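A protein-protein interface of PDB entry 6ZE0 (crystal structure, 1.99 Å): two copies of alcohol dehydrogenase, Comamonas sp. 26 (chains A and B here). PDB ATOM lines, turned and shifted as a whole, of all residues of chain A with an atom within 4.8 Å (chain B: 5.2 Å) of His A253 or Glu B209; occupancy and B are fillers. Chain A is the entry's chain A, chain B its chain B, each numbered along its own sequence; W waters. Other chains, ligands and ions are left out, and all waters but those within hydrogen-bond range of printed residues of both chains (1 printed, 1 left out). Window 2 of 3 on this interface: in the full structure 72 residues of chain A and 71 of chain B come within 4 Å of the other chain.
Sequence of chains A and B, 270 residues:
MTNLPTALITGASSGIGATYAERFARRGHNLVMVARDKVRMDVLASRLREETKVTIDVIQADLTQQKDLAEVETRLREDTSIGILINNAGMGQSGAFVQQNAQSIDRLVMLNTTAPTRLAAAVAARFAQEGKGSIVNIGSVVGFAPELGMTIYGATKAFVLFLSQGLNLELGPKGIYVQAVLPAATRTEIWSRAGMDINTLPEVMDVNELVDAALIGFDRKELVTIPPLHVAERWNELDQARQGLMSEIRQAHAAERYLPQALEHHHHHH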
ATOM      1  N   ARG A 250      -6.194  10.979  35.430  1.00  0.00           N
ATOM      2  CA  ARG A 250      -7.243  11.967  35.195  1.00  0.00           C
ATOM      3  C   ARG A 250      -8.137  11.414  34.094  1.00  0.00           C
ATOM      4  O   ARG A 250      -7.719  11.319  32.935  1.00  0.00           O
ATOM      5  CB  ARG A 250      -6.678  13.332  34.802  1.00  0.00           C
ATOM      6  CG  ARG A 250      -5.891  14.049  35.886  1.00  0.00           C
ATOM      7  CD  ARG A 250      -5.036  15.143  35.266  1.00  0.00           C
ATOM      8  NE  ARG A 250      -4.095  15.735  36.210  1.00  0.00           N
ATOM      9  CZ  ARG A 250      -3.537  16.932  36.055  1.00  0.00           C
ATOM     10  NH1 ARG A 250      -3.844  17.681  35.004  1.00  0.00           N
ATOM     11  NH2 ARG A 250      -2.682  17.387  36.957  1.00  0.00           N
ATOM     12  N   GLN A 251      -9.368  11.058  34.457  1.00  0.00           N
ATOM     13  CA  GLN A 251     -10.199  10.190  33.636  1.00  0.00           C
ATOM     14  C   GLN A 251     -11.058  10.927  32.616  1.00  0.00           C
ATOM     15  O   GLN A 251     -11.623  10.273  31.733  1.00  0.00           O
ATOM     16  CB  GLN A 251     -11.107   9.347  34.533  1.00  0.00           C
ATOM     17  CG  GLN A 251     -10.371   8.466  35.524  1.00  0.00           C
ATOM     18  CD  GLN A 251     -11.316   7.608  36.339  1.00  0.00           C
ATOM     19  OE1 GLN A 251     -11.588   6.459  35.993  1.00  0.00           O
ATOM     20  NE2 GLN A 251     -11.827   8.167  37.428  1.00  0.00           N
ATOM     21  N   ALA A 252     -11.176  12.254  32.706  1.00  0.00           N
ATOM     22  CA  ALA A 252     -12.090  12.967  31.816  1.00  0.00           C
ATOM     23  C   ALA A 252     -11.589  12.968  30.377  1.00  0.00           C
ATOM     24  O   ALA A 252     -12.373  12.772  29.441  1.00  0.00           O
ATOM     25  CB  ALA A 252     -12.301  14.397  32.309  1.00  0.00           C
ATOM     26  N   HIS A 253     -10.290  13.179  30.177  1.00  0.00           N
ATOM     27  CA  HIS A 253      -9.728  13.272  28.840  1.00  0.00           C
ATOM     28  C   HIS A 253      -8.384  12.561  28.805  1.00  0.00           C
ATOM     29  O   HIS A 253      -7.762  12.311  29.839  1.00  0.00           O
ATOM     30  CB  HIS A 253      -9.559  14.734  28.404  1.00  0.00           C
ATOM     31  CG  HIS A 253     -10.845  15.494  28.308  1.00  0.00           C
ATOM     32  ND1 HIS A 253     -11.746  15.309  27.281  1.00  0.00           N
ATOM     33  CD2 HIS A 253     -11.379  16.446  29.109  1.00  0.00           C
ATOM     34  CE1 HIS A 253     -12.780  16.112  27.455  1.00  0.00           C
ATOM     35  NE2 HIS A 253     -12.583  16.813  28.557  1.00  0.00           N
ATOM     36  N   ALA A 254      -7.940  12.236  27.594  1.00  0.00           N
ATOM     37  CA  ALA A 254      -6.618  11.658  27.416  1.00  0.00           C
ATOM     38  C   ALA A 254      -5.549  12.731  27.581  1.00  0.00           C
ATOM     39  O   ALA A 254      -5.778  13.913  27.314  1.00  0.00           O
ATOM     40  CB  ALA A 254      -6.501  11.002  26.040  1.00  0.00           C
ATOM     41  N   ALA A 255      -4.369  12.306  28.030  1.00  0.00           N
ATOM     42  CA  ALA A 255      -3.276  13.240  28.260  1.00  0.00           C
ATOM     43  C   ALA A 255      -2.863  13.912  26.952  1.00  0.00           C
ATOM     44  O   ALA A 255      -3.088  13.392  25.855  1.00  0.00           O
ATOM     45  CB  ALA A 255      -2.084  12.525  28.888  1.00  0.00           C
ATOM     46  N   MET B 205     -14.204   9.075  30.312  1.00  0.00           N
ATOM     47  CA  MET B 205     -13.717   9.496  29.012  1.00  0.00           C
ATOM     48  C   MET B 205     -14.625   8.972  27.912  1.00  0.00           C
ATOM     49  O   MET B 205     -15.109   7.837  27.977  1.00  0.00           O
ATOM     50  CB  MET B 205     -12.282   9.012  28.805  1.00  0.00           C
ATOM     51  CG  MET B 205     -11.640   9.479  27.521  1.00  0.00           C
ATOM     52  SD  MET B 205     -10.050   8.682  27.265  1.00  0.00           S
ATOM     53  CE  MET B 205      -9.236   9.069  28.815  1.00  0.00           C
ATOM     54  N   ASP B 206     -14.875   9.815  26.915  1.00  0.00           N
ATOM     55  CA  ASP B 206     -15.638   9.379  25.756  1.00  0.00           C
ATOM     56  C   ASP B 206     -14.901   8.229  25.082  1.00  0.00           C
ATOM     57  O   ASP B 206     -13.673   8.243  24.962  1.00  0.00           O
ATOM     58  CB  ASP B 206     -15.831  10.544  24.783  1.00  0.00           C
ATOM     59  CG  ASP B 206     -16.736  10.194  23.617  1.00  0.00           C
ATOM     60  OD1 ASP B 206     -17.338   9.100  23.628  1.00  0.00           O
ATOM     61  OD2 ASP B 206     -16.849  11.019  22.687  1.00  0.00           O
ATOM     62  N   VAL B 207     -15.661   7.218  24.654  1.00  0.00           N
ATOM     63  CA  VAL B 207     -15.043   6.034  24.064  1.00  0.00           C
ATOM     64  C   VAL B 207     -14.318   6.395  22.776  1.00  0.00           C
ATOM     65  O   VAL B 207     -13.299   5.780  22.433  1.00  0.00           O
ATOM     66  CB  VAL B 207     -16.098   4.931  23.843  1.00  0.00           C
ATOM     67  CG1 VAL B 207     -17.157   5.376  22.841  1.00  0.00           C
ATOM     68  CG2 VAL B 207     -15.434   3.636  23.401  1.00  0.00           C
ATOM     69  N   ASN B 208     -14.813   7.399  22.052  1.00  0.00           N
ATOM     70  CA  ASN B 208     -14.124   7.859  20.853  1.00  0.00           C
ATOM     71  C   ASN B 208     -12.775   8.480  21.198  1.00  0.00           C
ATOM     72  O   ASN B 208     -11.786   8.266  20.487  1.00  0.00           O
ATOM     73  CB  ASN B 208     -15.003   8.855  20.099  1.00  0.00           C
ATOM     74  CG  ASN B 208     -16.256   8.212  19.541  1.00  0.00           C
ATOM     75  OD1 ASN B 208     -16.215   7.527  18.516  1.00  0.00           O
ATOM     76  ND2 ASN B 208     -17.380   8.424  20.217  1.00  0.00           N
ATOM     77  N   GLU B 209     -12.715   9.259  22.279  1.00  0.00           N
ATOM     78  CA  GLU B 209     -11.445   9.847  22.690  1.00  0.00           C
ATOM     79  C   GLU B 209     -10.473   8.780  23.182  1.00  0.00           C
ATOM     80  O   GLU B 209      -9.264   8.878  22.944  1.00  0.00           O
ATOM     81  CB  GLU B 209     -11.682  10.905  23.767  1.00  0.00           C
ATOM     82  CG  GLU B 209     -10.416  11.591  24.243  1.00  0.00           C
ATOM     83  CD  GLU B 209     -10.696  12.798  25.116  1.00  0.00           C
ATOM     84  OE1 GLU B 209     -11.884  13.098  25.367  1.00  0.00           O
ATOM     85  OE2 GLU B 209      -9.723  13.450  25.545  1.00  0.00           O
ATOM     86  N   LEU B 210     -10.981   7.755  23.867  1.00  0.00           N
ATOM     87  CA  LEU B 210     -10.108   6.696  24.367  1.00  0.00           C
ATOM     88  C   LEU B 210      -9.475   5.911  23.225  1.00  0.00           C
ATOM     89  O   LEU B 210      -8.262   5.669  23.222  1.00  0.00           O
ATOM     90  CB  LEU B 210     -10.892   5.759  25.283  1.00  0.00           C
ATOM     91  CG  LEU B 210     -10.143   4.477  25.649  1.00  0.00           C
ATOM     92  CD1 LEU B 210      -8.972   4.780  26.577  1.00  0.00           C
ATOM     93  CD2 LEU B 210     -11.087   3.454  26.256  1.00  0.00           C
ATOM     94  N   VAL B 211     -10.282   5.507  22.242  1.00  0.00           N
ATOM     95  CA  VAL B 211      -9.761   4.691  21.151  1.00  0.00           C
ATOM     96  C   VAL B 211      -8.864   5.516  20.235  1.00  0.00           C
ATOM     97  O   VAL B 211      -7.864   5.005  19.712  1.00  0.00           O
ATOM     98  CB  VAL B 211     -10.924   4.035  20.383  1.00  0.00           C
ATOM     99  CG1 VAL B 211     -10.412   3.262  19.173  1.00  0.00           C
ATOM    100  CG2 VAL B 211     -11.707   3.117  21.310  1.00  0.00           C
ATOM    101  N   ASP B 212      -9.188   6.796  20.030  1.00  0.00           N
ATOM    102  CA  ASP B 212      -8.311   7.650  19.232  1.00  0.00           C
ATOM    103  C   ASP B 212      -6.940   7.791  19.882  1.00  0.00           C
ATOM    104  O   ASP B 212      -5.913   7.757  19.193  1.00  0.00           O
ATOM    105  CB  ASP B 212      -8.953   9.022  19.015  1.00  0.00           C
ATOM    106  CG  ASP B 212     -10.106   8.976  18.030  1.00  0.00           C
ATOM    107  OD1 ASP B 212     -10.221   7.971  17.295  1.00  0.00           O
ATOM    108  OD2 ASP B 212     -10.891   9.947  17.985  1.00  0.00           O
ATOM    109  N   ALA B 213      -6.903   7.956  21.205  1.00  0.00           N
ATOM    110  CA  ALA B 213      -5.626   7.978  21.908  1.00  0.00           C
ATOM    111  C   ALA B 213      -4.914   6.635  21.791  1.00  0.00           C
ATOM    112  O   ALA B 213      -3.694   6.585  21.596  1.00  0.00           O
ATOM    113  CB  ALA B 213      -5.839   8.349  23.376  1.00  0.00           C
ATOM    114  N   ALA B 214      -5.662   5.535  21.913  1.00  0.00           N
ATOM    115  CA  ALA B 214      -5.056   4.212  21.811  1.00  0.00           C
ATOM    116  C   ALA B 214      -4.494   3.952  20.419  1.00  0.00           C
ATOM    117  O   ALA B 214      -3.469   3.274  20.281  1.00  0.00           O
ATOM    118  CB  ALA B 214      -6.076   3.137  22.180  1.00  0.00           C
ATOM    119  N   PRO B 227      -4.048   6.203  28.299  1.00  0.00           N
ATOM    120  CA  PRO B 227      -4.504   7.555  27.920  1.00  0.00           C
ATOM    121  C   PRO B 227      -4.839   8.438  29.114  1.00  0.00           C
ATOM    122  O   PRO B 227      -4.465   9.621  29.111  1.00  0.00           O
ATOM    123  CB  PRO B 227      -5.744   7.274  27.056  1.00  0.00           C
ATOM    124  CG  PRO B 227      -5.465   5.937  26.455  1.00  0.00           C
ATOM    125  CD  PRO B 227      -4.725   5.154  27.515  1.00  0.00           C
ATOM    126  N   PRO B 228      -5.541   7.946  30.145  1.00  0.00           N
ATOM    127  CA  PRO B 228      -5.875   8.834  31.268  1.00  0.00           C
ATOM    128  C   PRO B 228      -4.725   9.112  32.225  1.00  0.00           C
ATOM    129  O   PRO B 228      -4.943   9.789  33.237  1.00  0.00           O
ATOM    130  CB  PRO B 228      -7.002   8.073  31.982  1.00  0.00           C
ATOM    131  CG  PRO B 228      -6.685   6.663  31.739  1.00  0.00           C
ATOM    132  CD  PRO B 228      -6.172   6.622  30.330  1.00  0.00           C
HETATM  133  O   HOH W   1     -13.903  12.554  26.586  1.00  0.00           O
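OE2 of Glu B209 sits at hydrogen-bond distance from N of Ala A254, 3.0 Å away.
N of Arg A250 is in hydrogen-bond range of O of Pro B228 (2.8 Å).
The side-chain carboxylate of Glu B209 sits at hydrogen-bond distance from a ring nitrogen (ND1) of His A253, at 2.9 Å.
The backbone carbonyl oxygen (O) of Gln A251 sits at hydrogen-bond distance from the backbone NH (N) of Met B205, at 3.2 Å.
O of Pro B227 lies within hydrogen-bond range of N of Ala A255 (2.9 Å).
The side-chain sulfur (SD) of Met B205 sits close to the backbone NH (N) of Leu B210, 3.6 Å away.
Ala A252 touches Met B205 (O to CA, 3.6 Å).
Met B205 touches His A253 (CE to C, 3.6 Å).
Ala A254 touches Met B205 (N to CE, 3.6 Å).
CB of Ala A254 touches CB of Ala B213, at 3.8 Å.
Ala A254 touches Pro B227.
His A253 touches just these residues of chain B: Met B205 (3.6 Å) and Glu B209 (2.9 Å).
Glu B209 touches just these residues of chain A: His A253 (2.9 Å) and Ala A254 (3.0 Å).
Printed residues of chain B within 4 Å of Ala A255: Pro B227.
Printed residues of chain B within 4 Å of Ala A254: Met B205, Glu B209, Ala B213 and Pro B227.
Of the printed residues of chain A, Pro B228 touches Arg A250.
Printed residues of chain B within 4 Å of Arg A250: Pro B228.
Of the printed residues of chain B, Gln A251 touches Met B205 (3.2 Å).
The nearest residue of chain A that does not touch Glu B209 is Ala A252 (4.1 Å).
The nearest printed residue of chain A that does not touch Pro B227 is His A253 (4.3 Å).
Hydrophobic or aromatic side chains of chain B that line the printed part of chain A: Met B205, Ala B213, Pro B227 and Pro B228.
Hydrophobic or aromatic side chains of chain A within 4 Å of the printed part of chain B: His A253, Ala A254 and Ala A255.
Along chain A the printed residues that touch a printed residue of chain B span positions 250 to 255.
Among the printed residues, 10 pairs touch across the chains.
Among the printed residues, no Asp or Glu carboxylate lies within 4 Å of a Lys or Arg side-chain nitrogen of the other chain.
No position is printed for both chains.
Of the 10 pairs that touch across the chains among the printed residues, none has its exchanged pair printed and touching as well.
Water W1 lies within hydrogen-bond range of OE1 of Glu B209 (2.4 Å), N of Asp B206 (2.9 Å) and O of Ala A252 (3.2 Å).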
